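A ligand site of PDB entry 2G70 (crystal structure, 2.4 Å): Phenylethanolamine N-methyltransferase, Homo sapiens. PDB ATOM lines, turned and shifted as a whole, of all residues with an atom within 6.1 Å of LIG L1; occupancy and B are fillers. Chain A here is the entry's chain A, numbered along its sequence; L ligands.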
ATOM      1  N   VAL A  23     -25.529  15.809  -7.255  1.00  0.00           N
ATOM      2  CA  VAL A  23     -25.166  15.732  -5.844  1.00  0.00           C
ATOM      3  C   VAL A  23     -25.059  17.113  -5.216  1.00  0.00           C
ATOM      4  O   VAL A  23     -25.877  17.485  -4.378  1.00  0.00           O
ATOM      5  CB  VAL A  23     -23.826  14.975  -5.657  1.00  0.00           C
ATOM      6  CG1 VAL A  23     -23.480  14.884  -4.187  1.00  0.00           C
ATOM      7  CG2 VAL A  23     -23.919  13.582  -6.264  1.00  0.00           C
ATOM      8  N   ALA A  24     -24.048  17.879  -5.620  1.00  0.00           N
ATOM      9  CA  ALA A  24     -23.835  19.217  -5.092  1.00  0.00           C
ATOM     10  C   ALA A  24     -25.114  20.063  -5.186  1.00  0.00           C
ATOM     11  O   ALA A  24     -25.319  20.985  -4.386  1.00  0.00           O
ATOM     12  CB  ALA A  24     -22.694  19.902  -5.833  1.00  0.00           C
ATOM     13  N   TYR A  27     -27.595  19.098  -2.110  1.00  0.00           N
ATOM     14  CA  TYR A  27     -27.176  19.619  -0.808  1.00  0.00           C
ATOM     15  C   TYR A  27     -27.424  21.119  -0.617  1.00  0.00           C
ATOM     16  O   TYR A  27     -27.166  21.661   0.449  1.00  0.00           O
ATOM     17  CB  TYR A  27     -25.700  19.315  -0.537  1.00  0.00           C
ATOM     18  CG  TYR A  27     -25.447  17.883  -0.107  1.00  0.00           C
ATOM     19  CD1 TYR A  27     -25.047  16.912  -1.028  1.00  0.00           C
ATOM     20  CD2 TYR A  27     -25.642  17.499   1.217  1.00  0.00           C
ATOM     21  CE1 TYR A  27     -24.859  15.585  -0.638  1.00  0.00           C
ATOM     22  CE2 TYR A  27     -25.462  16.178   1.617  1.00  0.00           C
ATOM     23  CZ  TYR A  27     -25.071  15.227   0.683  1.00  0.00           C
ATOM     24  OH  TYR A  27     -24.873  13.930   1.083  1.00  0.00           O
ATOM     25  N   PHE A  30     -30.048  21.169   1.864  1.00  0.00           N
ATOM     26  CA  PHE A  30     -29.677  20.502   3.118  1.00  0.00           C
ATOM     27  C   PHE A  30     -29.810  21.442   4.305  1.00  0.00           C
ATOM     28  O   PHE A  30     -29.195  22.500   4.328  1.00  0.00           O
ATOM     29  CB  PHE A  30     -28.235  20.004   3.013  1.00  0.00           C
ATOM     30  CG  PHE A  30     -27.773  19.201   4.209  1.00  0.00           C
ATOM     31  CD1 PHE A  30     -27.719  17.816   4.148  1.00  0.00           C
ATOM     32  CD2 PHE A  30     -27.392  19.848   5.382  1.00  0.00           C
ATOM     33  CE1 PHE A  30     -27.281  17.061   5.231  1.00  0.00           C
ATOM     34  CE2 PHE A  30     -26.952  19.116   6.484  1.00  0.00           C
ATOM     35  CZ  PHE A  30     -26.896  17.716   6.414  1.00  0.00           C
ATOM     36  N   TYR A  35     -31.209  17.699  10.077  1.00  0.00           N
ATOM     37  CA  TYR A  35     -30.308  16.569  10.029  1.00  0.00           C
ATOM     38  C   TYR A  35     -29.949  16.136  11.454  1.00  0.00           C
ATOM     39  O   TYR A  35     -29.927  14.944  11.774  1.00  0.00           O
ATOM     40  CB  TYR A  35     -29.038  16.947   9.271  1.00  0.00           C
ATOM     41  CG  TYR A  35     -28.019  15.838   9.243  1.00  0.00           C
ATOM     42  CD1 TYR A  35     -28.112  14.801   8.321  1.00  0.00           C
ATOM     43  CD2 TYR A  35     -26.964  15.826  10.149  1.00  0.00           C
ATOM     44  CE1 TYR A  35     -27.190  13.782   8.311  1.00  0.00           C
ATOM     45  CE2 TYR A  35     -26.036  14.815  10.139  1.00  0.00           C
ATOM     46  CZ  TYR A  35     -26.154  13.797   9.234  1.00  0.00           C
ATOM     47  OH  TYR A  35     -25.228  12.787   9.254  1.00  0.00           O
ATOM     48  N   ASN A  39     -30.887  12.440  13.225  1.00  0.00           N
ATOM     49  CA  ASN A  39     -29.876  11.455  13.563  1.00  0.00           C
ATOM     50  C   ASN A  39     -29.225  11.584  14.920  1.00  0.00           C
ATOM     51  O   ASN A  39     -28.504  10.687  15.360  1.00  0.00           O
ATOM     52  CB  ASN A  39     -28.780  11.493  12.511  1.00  0.00           C
ATOM     53  CG  ASN A  39     -29.283  11.130  11.146  1.00  0.00           C
ATOM     54  OD1 ASN A  39     -29.631   9.969  10.890  1.00  0.00           O
ATOM     55  ND2 ASN A  39     -29.313  12.116  10.261  1.00  0.00           N
ATOM     56  N   TYR A  40     -29.436  12.705  15.601  1.00  0.00           N
ATOM     57  CA  TYR A  40     -28.787  12.852  16.888  1.00  0.00           C
ATOM     58  C   TYR A  40     -29.680  13.288  18.018  1.00  0.00           C
ATOM     59  O   TYR A  40     -29.211  13.766  19.045  1.00  0.00           O
ATOM     60  CB  TYR A  40     -27.576  13.745  16.737  1.00  0.00           C
ATOM     61  CG  TYR A  40     -26.600  13.162  15.750  1.00  0.00           C
ATOM     62  CD1 TYR A  40     -26.646  13.483  14.397  1.00  0.00           C
ATOM     63  CD2 TYR A  40     -25.620  12.249  16.183  1.00  0.00           C
ATOM     64  CE1 TYR A  40     -25.763  12.907  13.482  1.00  0.00           C
ATOM     65  CE2 TYR A  40     -24.731  11.668  15.289  1.00  0.00           C
ATOM     66  CZ  TYR A  40     -24.802  12.008  13.953  1.00  0.00           C
ATOM     67  OH  TYR A  40     -23.921  11.420  13.079  1.00  0.00           O
ATOM     68  N   LYS A  57     -20.939   3.785  18.109  1.00  0.00           N
ATOM     69  CA  LYS A  57     -19.979   4.639  17.436  1.00  0.00           C
ATOM     70  C   LYS A  57     -18.935   5.170  18.420  1.00  0.00           C
ATOM     71  O   LYS A  57     -17.733   5.088  18.156  1.00  0.00           O
ATOM     72  CB  LYS A  57     -20.678   5.796  16.717  1.00  0.00           C
ATOM     73  CG  LYS A  57     -21.109   5.480  15.285  1.00  0.00           C
ATOM     74  CD  LYS A  57     -21.760   6.687  14.608  1.00  0.00           C
ATOM     75  CE  LYS A  57     -23.015   7.143  15.355  1.00  0.00           C
ATOM     76  NZ  LYS A  57     -23.589   8.437  14.842  1.00  0.00           N
ATOM     77  N   ASP A  77     -10.735  16.327   9.967  1.00  0.00           N
ATOM     78  CA  ASP A  77     -12.031  15.673   9.950  1.00  0.00           C
ATOM     79  C   ASP A  77     -12.642  15.960   8.579  1.00  0.00           C
ATOM     80  O   ASP A  77     -12.953  17.115   8.266  1.00  0.00           O
ATOM     81  CB  ASP A  77     -12.895  16.240  11.088  1.00  0.00           C
ATOM     82  CG  ASP A  77     -14.260  15.612  11.174  1.00  0.00           C
ATOM     83  OD1 ASP A  77     -14.374  14.392  10.931  1.00  0.00           O
ATOM     84  OD2 ASP A  77     -15.230  16.328  11.493  1.00  0.00           O
ATOM     85  N   ILE A  78     -12.793  14.928   7.753  1.00  0.00           N
ATOM     86  CA  ILE A  78     -13.355  15.072   6.412  1.00  0.00           C
ATOM     87  C   ILE A  78     -14.882  14.986   6.433  1.00  0.00           C
ATOM     88  O   ILE A  78     -15.451  14.017   6.944  1.00  0.00           O
ATOM     89  CB  ILE A  78     -12.818  13.980   5.457  1.00  0.00           C
ATOM     90  CG1 ILE A  78     -11.405  14.324   4.994  1.00  0.00           C
ATOM     91  CG2 ILE A  78     -13.725  13.859   4.248  1.00  0.00           C
ATOM     92  CD1 ILE A  78     -10.376  14.339   6.088  1.00  0.00           C
ATOM     93  N   GLY A  79     -15.540  15.991   5.854  1.00  0.00           N
ATOM     94  CA  GLY A  79     -16.985  15.982   5.819  1.00  0.00           C
ATOM     95  C   GLY A  79     -17.528  15.900   7.231  1.00  0.00           C
ATOM     96  O   GLY A  79     -17.981  14.839   7.666  1.00  0.00           O
ATOM     97  N   SER A  80     -17.492  17.027   7.934  1.00  0.00           N
ATOM     98  CA  SER A  80     -17.950  17.109   9.307  1.00  0.00           C
ATOM     99  C   SER A  80     -19.435  17.383   9.458  1.00  0.00           C
ATOM    100  O   SER A  80     -20.069  16.875  10.387  1.00  0.00           O
ATOM    101  CB  SER A  80     -17.201  18.216  10.052  1.00  0.00           C
ATOM    102  OG  SER A  80     -15.809  18.121   9.845  1.00  0.00           O
ATOM    103  N   GLY A  81     -19.987  18.184   8.565  1.00  0.00           N
ATOM    104  CA  GLY A  81     -21.384  18.529   8.670  1.00  0.00           C
ATOM    105  C   GLY A  81     -21.572  19.319   9.959  1.00  0.00           C
ATOM    106  O   GLY A  81     -20.652  20.031  10.383  1.00  0.00           O
ATOM    107  N   PRO A  82     -22.736  19.218  10.615  1.00  0.00           N
ATOM    108  CA  PRO A  82     -22.938  19.969  11.864  1.00  0.00           C
ATOM    109  C   PRO A  82     -22.626  19.182  13.137  1.00  0.00           C
ATOM    110  O   PRO A  82     -22.993  19.609  14.234  1.00  0.00           O
ATOM    111  CB  PRO A  82     -24.416  20.360  11.770  1.00  0.00           C
ATOM    112  CG  PRO A  82     -25.022  19.174  11.121  1.00  0.00           C
ATOM    113  CD  PRO A  82     -24.034  18.814  10.025  1.00  0.00           C
ATOM    114  N   THR A  83     -21.932  18.055  13.011  1.00  0.00           N
ATOM    115  CA  THR A  83     -21.612  17.213  14.167  1.00  0.00           C
ATOM    116  C   THR A  83     -20.161  17.267  14.673  1.00  0.00           C
ATOM    117  O   THR A  83     -19.229  17.480  13.912  1.00  0.00           O
ATOM    118  CB  THR A  83     -21.945  15.746  13.874  1.00  0.00           C
ATOM    119  OG1 THR A  83     -20.968  15.223  12.965  1.00  0.00           O
ATOM    120  CG2 THR A  83     -23.313  15.617  13.238  1.00  0.00           C
ATOM    121  N   TYR A  85     -19.472  15.010  17.685  1.00  0.00           N
ATOM    122  CA  TYR A  85     -19.348  13.749  18.418  1.00  0.00           C
ATOM    123  C   TYR A  85     -18.202  12.873  17.920  1.00  0.00           C
ATOM    124  O   TYR A  85     -17.510  12.232  18.719  1.00  0.00           O
ATOM    125  CB  TYR A  85     -20.680  12.946  18.354  1.00  0.00           C
ATOM    126  CG  TYR A  85     -20.841  12.127  17.096  1.00  0.00           C
ATOM    127  CD1 TYR A  85     -20.263  10.874  16.985  1.00  0.00           C
ATOM    128  CD2 TYR A  85     -21.507  12.642  15.983  1.00  0.00           C
ATOM    129  CE1 TYR A  85     -20.326  10.154  15.792  1.00  0.00           C
ATOM    130  CE2 TYR A  85     -21.586  11.935  14.799  1.00  0.00           C
ATOM    131  CZ  TYR A  85     -20.997  10.698  14.708  1.00  0.00           C
ATOM    132  OH  TYR A  85     -21.050  10.008  13.515  1.00  0.00           O
ATOM    133  N   GLN A  86     -17.978  12.862  16.614  1.00  0.00           N
ATOM    134  CA  GLN A  86     -16.924  12.050  16.014  1.00  0.00           C
ATOM    135  C   GLN A  86     -15.492  12.417  16.426  1.00  0.00           C
ATOM    136  O   GLN A  86     -14.535  11.727  16.065  1.00  0.00           O
ATOM    137  CB  GLN A  86     -17.043  12.076  14.486  1.00  0.00           C
ATOM    138  CG  GLN A  86     -16.752  13.438  13.865  1.00  0.00           C
ATOM    139  CD  GLN A  86     -17.990  14.316  13.753  1.00  0.00           C
ATOM    140  OE1 GLN A  86     -18.882  14.261  14.601  1.00  0.00           O
ATOM    141  NE2 GLN A  86     -18.040  15.143  12.711  1.00  0.00           N
ATOM    142  N   ASP A 101     -16.144  20.920   5.778  1.00  0.00           N
ATOM    143  CA  ASP A 101     -17.450  20.651   5.193  1.00  0.00           C
ATOM    144  C   ASP A 101     -17.734  21.529   3.978  1.00  0.00           C
ATOM    145  O   ASP A 101     -17.332  22.695   3.927  1.00  0.00           O
ATOM    146  CB  ASP A 101     -18.580  20.806   6.213  1.00  0.00           C
ATOM    147  CG  ASP A 101     -19.831  20.052   5.792  1.00  0.00           C
ATOM    148  OD1 ASP A 101     -19.741  18.820   5.588  1.00  0.00           O
ATOM    149  OD2 ASP A 101     -20.905  20.684   5.654  1.00  0.00           O
ATOM    150  N   PHE A 102     -18.454  20.956   3.024  1.00  0.00           N
ATOM    151  CA  PHE A 102     -18.815  21.603   1.762  1.00  0.00           C
ATOM    152  C   PHE A 102     -19.782  22.771   1.852  1.00  0.00           C
ATOM    153  O   PHE A 102     -19.784  23.632   0.975  1.00  0.00           O
ATOM    154  CB  PHE A 102     -19.412  20.546   0.827  1.00  0.00           C
ATOM    155  CG  PHE A 102     -19.522  20.985  -0.596  1.00  0.00           C
ATOM    156  CD1 PHE A 102     -18.404  20.987  -1.423  1.00  0.00           C
ATOM    157  CD2 PHE A 102     -20.750  21.381  -1.131  1.00  0.00           C
ATOM    158  CE1 PHE A 102     -18.494  21.368  -2.752  1.00  0.00           C
ATOM    159  CE2 PHE A 102     -20.854  21.761  -2.461  1.00  0.00           C
ATOM    160  CZ  PHE A 102     -19.729  21.757  -3.277  1.00  0.00           C
ATOM    161  N   LEU A 103     -20.615  22.816   2.883  1.00  0.00           N
ATOM    162  CA  LEU A 103     -21.587  23.885   2.997  1.00  0.00           C
ATOM    163  C   LEU A 103     -21.347  24.863   4.125  1.00  0.00           C
ATOM    164  O   LEU A 103     -21.206  24.471   5.278  1.00  0.00           O
ATOM    165  CB  LEU A 103     -22.992  23.313   3.159  1.00  0.00           C
ATOM    166  CG  LEU A 103     -23.483  22.210   2.215  1.00  0.00           C
ATOM    167  CD1 LEU A 103     -24.959  21.959   2.528  1.00  0.00           C
ATOM    168  CD2 LEU A 103     -23.296  22.630   0.768  1.00  0.00           C
ATOM    169  N   ASN A 106     -23.260  24.402   7.241  1.00  0.00           N
ATOM    170  CA  ASN A 106     -22.800  23.453   8.233  1.00  0.00           C
ATOM    171  C   ASN A 106     -21.649  24.058   9.033  1.00  0.00           C
ATOM    172  O   ASN A 106     -21.557  23.871  10.253  1.00  0.00           O
ATOM    173  CB  ASN A 106     -22.349  22.139   7.590  1.00  0.00           C
ATOM    174  CG  ASN A 106     -23.511  21.248   7.223  1.00  0.00           C
ATOM    175  OD1 ASN A 106     -24.547  21.275   7.885  1.00  0.00           O
ATOM    176  ND2 ASN A 106     -23.341  20.426   6.195  1.00  0.00           N
ATOM    177  N   ILE A 157     -14.303  22.056   1.755  1.00  0.00           N
ATOM    178  CA  ILE A 157     -13.646  20.908   1.145  1.00  0.00           C
ATOM    179  C   ILE A 157     -14.583  20.280   0.123  1.00  0.00           C
ATOM    180  O   ILE A 157     -15.795  20.479   0.181  1.00  0.00           O
ATOM    181  CB  ILE A 157     -13.253  19.857   2.225  1.00  0.00           C
ATOM    182  CG1 ILE A 157     -12.590  18.642   1.557  1.00  0.00           C
ATOM    183  CG2 ILE A 157     -14.471  19.436   3.019  1.00  0.00           C
ATOM    184  CD1 ILE A 157     -12.183  17.545   2.529  1.00  0.00           C
ATOM    185  N   ASP A 158     -14.001  19.549  -0.822  1.00  0.00           N
ATOM    186  CA  ASP A 158     -14.753  18.875  -1.866  1.00  0.00           C
ATOM    187  C   ASP A 158     -13.974  17.608  -2.140  1.00  0.00           C
ATOM    188  O   ASP A 158     -13.033  17.621  -2.922  1.00  0.00           O
ATOM    189  CB  ASP A 158     -14.802  19.734  -3.129  1.00  0.00           C
ATOM    190  CG  ASP A 158     -15.641  19.119  -4.243  1.00  0.00           C
ATOM    191  OD1 ASP A 158     -15.488  17.904  -4.523  1.00  0.00           O
ATOM    192  OD2 ASP A 158     -16.460  19.856  -4.836  1.00  0.00           O
ATOM    193  N   VAL A 159     -14.363  16.515  -1.488  1.00  0.00           N
ATOM    194  CA  VAL A 159     -13.657  15.251  -1.658  1.00  0.00           C
ATOM    195  C   VAL A 159     -13.576  14.769  -3.108  1.00  0.00           C
ATOM    196  O   VAL A 159     -12.858  13.807  -3.400  1.00  0.00           O
ATOM    197  CB  VAL A 159     -14.288  14.129  -0.795  1.00  0.00           C
ATOM    198  CG1 VAL A 159     -14.247  14.525   0.670  1.00  0.00           C
ATOM    199  CG2 VAL A 159     -15.713  13.860  -1.240  1.00  0.00           C
ATOM    200  N   HIS A 160     -14.303  15.430  -4.011  1.00  0.00           N
ATOM    201  CA  HIS A 160     -14.278  15.029  -5.420  1.00  0.00           C
ATOM    202  C   HIS A 160     -13.141  15.669  -6.220  1.00  0.00           C
ATOM    203  O   HIS A 160     -12.834  15.214  -7.331  1.00  0.00           O
ATOM    204  CB  HIS A 160     -15.633  15.313  -6.082  1.00  0.00           C
ATOM    205  CG  HIS A 160     -16.715  14.385  -5.627  1.00  0.00           C
ATOM    206  ND1 HIS A 160     -16.579  13.009  -5.672  1.00  0.00           N
ATOM    207  CD2 HIS A 160     -17.936  14.628  -5.100  1.00  0.00           C
ATOM    208  CE1 HIS A 160     -17.678  12.451  -5.183  1.00  0.00           C
ATOM    209  NE2 HIS A 160     -18.507  13.411  -4.831  1.00  0.00           N
ATOM    210  N   ALA A 181     -16.835  10.554   8.949  1.00  0.00           N
ATOM    211  CA  ALA A 181     -18.055   9.841   9.302  1.00  0.00           C
ATOM    212  C   ALA A 181     -19.252  10.247   8.459  1.00  0.00           C
ATOM    213  O   ALA A 181     -19.646  11.421   8.438  1.00  0.00           O
ATOM    214  CB  ALA A 181     -18.368  10.086  10.772  1.00  0.00           C
ATOM    215  N   PHE A 182     -19.835   9.275   7.773  1.00  0.00           N
ATOM    216  CA  PHE A 182     -21.019   9.491   6.938  1.00  0.00           C
ATOM    217  C   PHE A 182     -20.818  10.542   5.849  1.00  0.00           C
ATOM    218  O   PHE A 182     -21.711  11.353   5.619  1.00  0.00           O
ATOM    219  CB  PHE A 182     -22.200   9.897   7.814  1.00  0.00           C
ATOM    220  CG  PHE A 182     -22.620   8.845   8.793  1.00  0.00           C
ATOM    221  CD1 PHE A 182     -22.612   9.105  10.149  1.00  0.00           C
ATOM    222  CD2 PHE A 182     -23.007   7.593   8.346  1.00  0.00           C
ATOM    223  CE1 PHE A 182     -22.976   8.113  11.061  1.00  0.00           C
ATOM    224  CE2 PHE A 182     -23.368   6.586   9.248  1.00  0.00           C
ATOM    225  CZ  PHE A 182     -23.360   6.846  10.605  1.00  0.00           C
ATOM    226  N   CYS A 183     -19.681  10.525   5.166  1.00  0.00           N
ATOM    227  CA  CYS A 183     -19.456  11.516   4.122  1.00  0.00           C
ATOM    228  C   CYS A 183     -19.290  10.939   2.722  1.00  0.00           C
ATOM    229  O   CYS A 183     -20.134  11.140   1.857  1.00  0.00           O
ATOM    230  CB  CYS A 183     -18.236  12.362   4.446  1.00  0.00           C
ATOM    231  SG  CYS A 183     -17.800  13.527   3.122  1.00  0.00           S
ATOM    232  N   ALA A 186     -22.199   9.277   1.218  1.00  0.00           N
ATOM    233  CA  ALA A 186     -23.313  10.221   1.154  1.00  0.00           C
ATOM    234  C   ALA A 186     -23.156  11.318   0.090  1.00  0.00           C
ATOM    235  O   ALA A 186     -24.093  12.088  -0.153  1.00  0.00           O
ATOM    236  CB  ALA A 186     -23.540  10.847   2.526  1.00  0.00           C
ATOM    237  N   VAL A 187     -21.991  11.392  -0.545  1.00  0.00           N
ATOM    238  CA  VAL A 187     -21.781  12.434  -1.552  1.00  0.00           C
ATOM    239  C   VAL A 187     -21.311  11.906  -2.897  1.00  0.00           C
ATOM    240  O   VAL A 187     -20.981  12.682  -3.792  1.00  0.00           O
ATOM    241  CB  VAL A 187     -20.762  13.486  -1.062  1.00  0.00           C
ATOM    242  CG1 VAL A 187     -21.229  14.063   0.260  1.00  0.00           C
ATOM    243  CG2 VAL A 187     -19.383  12.853  -0.907  1.00  0.00           C
ATOM    244  N   TYR A 222     -31.443   9.658   2.236  1.00  0.00           N
ATOM    245  CA  TYR A 222     -31.738  10.161   3.566  1.00  0.00           C
ATOM    246  C   TYR A 222     -32.285  11.576   3.423  1.00  0.00           C
ATOM    247  O   TYR A 222     -32.000  12.249   2.437  1.00  0.00           O
ATOM    248  CB  TYR A 222     -30.495  10.139   4.449  1.00  0.00           C
ATOM    249  CG  TYR A 222     -29.461  11.204   4.146  1.00  0.00           C
ATOM    250  CD1 TYR A 222     -29.586  12.491   4.677  1.00  0.00           C
ATOM    251  CD2 TYR A 222     -28.350  10.916   3.360  1.00  0.00           C
ATOM    252  CE1 TYR A 222     -28.631  13.452   4.441  1.00  0.00           C
ATOM    253  CE2 TYR A 222     -27.380  11.877   3.105  1.00  0.00           C
ATOM    254  CZ  TYR A 222     -27.525  13.141   3.656  1.00  0.00           C
ATOM    255  OH  TYR A 222     -26.580  14.109   3.429  1.00  0.00           O
HETATM  256  N1  LIG L   1     -20.159  14.024   9.647  1.00  0.00           N
HETATM  257  C1  LIG L   1     -21.538  14.203  10.103  1.00  0.00           C
HETATM  258  C2  LIG L   1     -22.056  13.005  10.919  1.00  0.00           C
HETATM  259  O1  LIG L   1     -21.208  12.209  11.406  1.00  0.00           O
HETATM  260  O2  LIG L   1     -23.280  12.889  11.108  1.00  0.00           O
HETATM  261  C3  LIG L   1     -22.454  14.537   8.895  1.00  0.00           C
HETATM  262  C4  LIG L   1     -22.376  13.602   7.673  1.00  0.00           C
HETATM  263  S1  LIG L   1     -23.478  14.142   6.280  1.00  0.00           S
HETATM  264  C5  LIG L   1     -24.706  12.904   5.970  1.00  0.00           C
HETATM  265  C6  LIG L   1     -22.525  14.439   4.714  1.00  0.00           C
HETATM  266  C7  LIG L   1     -21.745  15.738   4.660  1.00  0.00           C
HETATM  267  O3  LIG L   1     -20.932  15.867   3.460  1.00  0.00           O
HETATM  268  C8  LIG L   1     -22.651  16.974   4.703  1.00  0.00           C
HETATM  269  O4  LIG L   1     -22.265  17.823   5.788  1.00  0.00           O
HETATM  270  C9  LIG L   1     -22.434  17.636   3.340  1.00  0.00           C
HETATM  271  O5  LIG L   1     -22.516  19.045   3.358  1.00  0.00           O
HETATM  272  C10 LIG L   1     -21.009  17.197   3.009  1.00  0.00           C
HETATM  273  N2  LIG L   1     -20.668  17.250   1.580  1.00  0.00           N
HETATM  274  C11 LIG L   1     -21.521  17.531   0.470  1.00  0.00           C
HETATM  275  N3  LIG L   1     -20.891  17.536  -0.680  1.00  0.00           N
HETATM  276  C12 LIG L   1     -19.581  17.246  -0.334  1.00  0.00           C
HETATM  277  C13 LIG L   1     -18.442  17.129  -1.164  1.00  0.00           C
HETATM  278  N4  LIG L   1     -18.465  17.290  -2.488  1.00  0.00           N
HETATM  279  N5  LIG L   1     -17.246  16.846  -0.567  1.00  0.00           N
HETATM  280  C14 LIG L   1     -17.226  16.686   0.788  1.00  0.00           C
HETATM  281  N6  LIG L   1     -18.251  16.775   1.669  1.00  0.00           N
HETATM  282  C15 LIG L   1     -19.410  17.067   1.034  1.00  0.00           C
HETATM  283  C1  LG2 L   2     -26.132  10.027   8.390  1.00  0.00           C
HETATM  284  C2  LG2 L   2     -26.230   9.143   7.140  1.00  0.00           C
HETATM  285  O1  LG2 L   2     -27.832   5.714  12.952  1.00  0.00           O
HETATM  286  C3  LG2 L   2     -27.569   7.391   8.188  1.00  0.00           C
HETATM  287  C4  LG2 L   2     -27.311   7.198  10.679  1.00  0.00           C
HETATM  288  C5  LG2 L   2     -26.872   7.655  11.915  1.00  0.00           C
HETATM  289  C6  LG2 L   2     -26.194   8.865  12.006  1.00  0.00           C
HETATM  290  C7  LG2 L   2     -25.969   9.616  10.851  1.00  0.00           C
HETATM  291  O2  LG2 L   2     -25.764   9.100   4.772  1.00  0.00           O
HETATM  292  C8  LG2 L   2     -26.046   9.970   5.868  1.00  0.00           C
HETATM  293  C9  LG2 L   2     -26.401   9.167   9.616  1.00  0.00           C
HETATM  294  N1  LG2 L   2     -27.150   6.960  13.023  1.00  0.00           N
HETATM  295  O3  LG2 L   2     -26.769   7.462  14.302  1.00  0.00           O
HETATM  296  C10 LG2 L   2     -27.071   7.951   9.525  1.00  0.00           C
HETATM  297  N2  LG2 L   2     -27.513   8.428   7.137  1.00  0.00           N
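The backbone carbonyl oxygen of Phe 182 sits close to a sulfur (S1) of LIG L1, 3.4 Å away.
Tyr 27 touches LIG L1 (CE2 to C9, 3.8 Å).
Gly 81 touches LIG L1 (CA to O4, 3.1 Å).
Gln 86 touches LIG L1 (NE2 to N1, 3.9 Å).
CB of Phe 102 touches C15 of LIG L1, 3.5 Å away.
CG of Leu 103 touches O5 of LIG L1, 3.5 Å away.
Ile 157 touches LIG L1 (O to N5, 3.98 Å).
CA of Asp 158 touches N5 of LIG L1, at 3.5 Å.
His 160 touches LIG L1 (CD2 to N4, 3.8 Å).
Val 187 touches LIG L1.
OH of Tyr 222 touches C5 of LIG L1 (3.4 Å).
Hydrophobic or aromatic side chains that line LIG L1: Tyr 27, Tyr 35, Tyr 40, Tyr 85, Phe 102, Leu 103, Val 159, His 160, Ala 181, Phe 182, Val 187 and Tyr 222.
Of the 31 residues printed, 22 come within 4 Å of LIG L1.
OH of Tyr 40 sits close to OH of Tyr 85, at 3.2 Å.
The side-chain amino group (NZ) of Lys 57 sits close to the side-chain hydroxyl (OH) of Tyr 40 (3.5 Å).
ND2 of Asn 39 is in hydrogen-bond range of O of Tyr 35 (3.3 Å).
The side-chain carboxylate (OD2) of Asp 101 lies within hydrogen-bond range of the side-chain amide nitrogen (ND2) of Asn 106 (2.5 Å).
The backbone carbonyl oxygen (O) of Ser 80 sits at hydrogen-bond distance from the side-chain hydroxyl (OG1) of Thr 83, 3.2 Å away.
The side-chain hydroxyl (OH) of Tyr 85 is in hydrogen-bond range of the side-chain amino group (NZ) of Lys 57, at 3.3 Å.
OE1 of Gln 86 lies within hydrogen-bond range of OG1 of Thr 83, 2.8 Å away.
The side-chain hydroxyl (OH) of Tyr 222 sits at hydrogen-bond distance from the side-chain hydroxyl (OH) of Tyr 27 (2.9 Å).
O2 of LIG L1 is in hydrogen-bond range of OH of Tyr 40 (2.5 Å).
An oxygen (O2) of LIG L1 sits at hydrogen-bond distance from the side-chain hydroxyl (OH) of Tyr 35 (2.7 Å).
An oxygen (O4) of LIG L1 sits at hydrogen-bond distance from the side-chain carboxylate of Asp 101.
ND2 of Asn 106 is in hydrogen-bond range of O4 of LIG L1.
O of Ala 181 sits at hydrogen-bond distance from N1 of LIG L1, 2.9 Å away.
O of Ser 80 sits at hydrogen-bond distance from N1 of LIG L1 (2.9 Å).
The backbone NH (N) of Val 159 lies within hydrogen-bond range of a nitrogen (N5) of LIG L1, at 3.0 Å.
An oxygen (O1) of LIG L1 is in hydrogen-bond range of the side-chain hydroxyl of Tyr 85 (3.1 Å).
A nitrogen (N1) of LIG L1 lies within hydrogen-bond range of the backbone carbonyl oxygen of Gly 79.
The side-chain hydroxyl of Thr 83 lies close to an oxygen (O1) of LIG L1 (3.4 Å).
SG of Cys 183 lies within hydrogen-bond range of N6 of LIG L1 (3.6 Å).
The side-chain amino group (NZ) of Lys 57 sits at hydrogen-bond distance from an oxygen (O3) of LG2 L2, 3.4 Å away.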
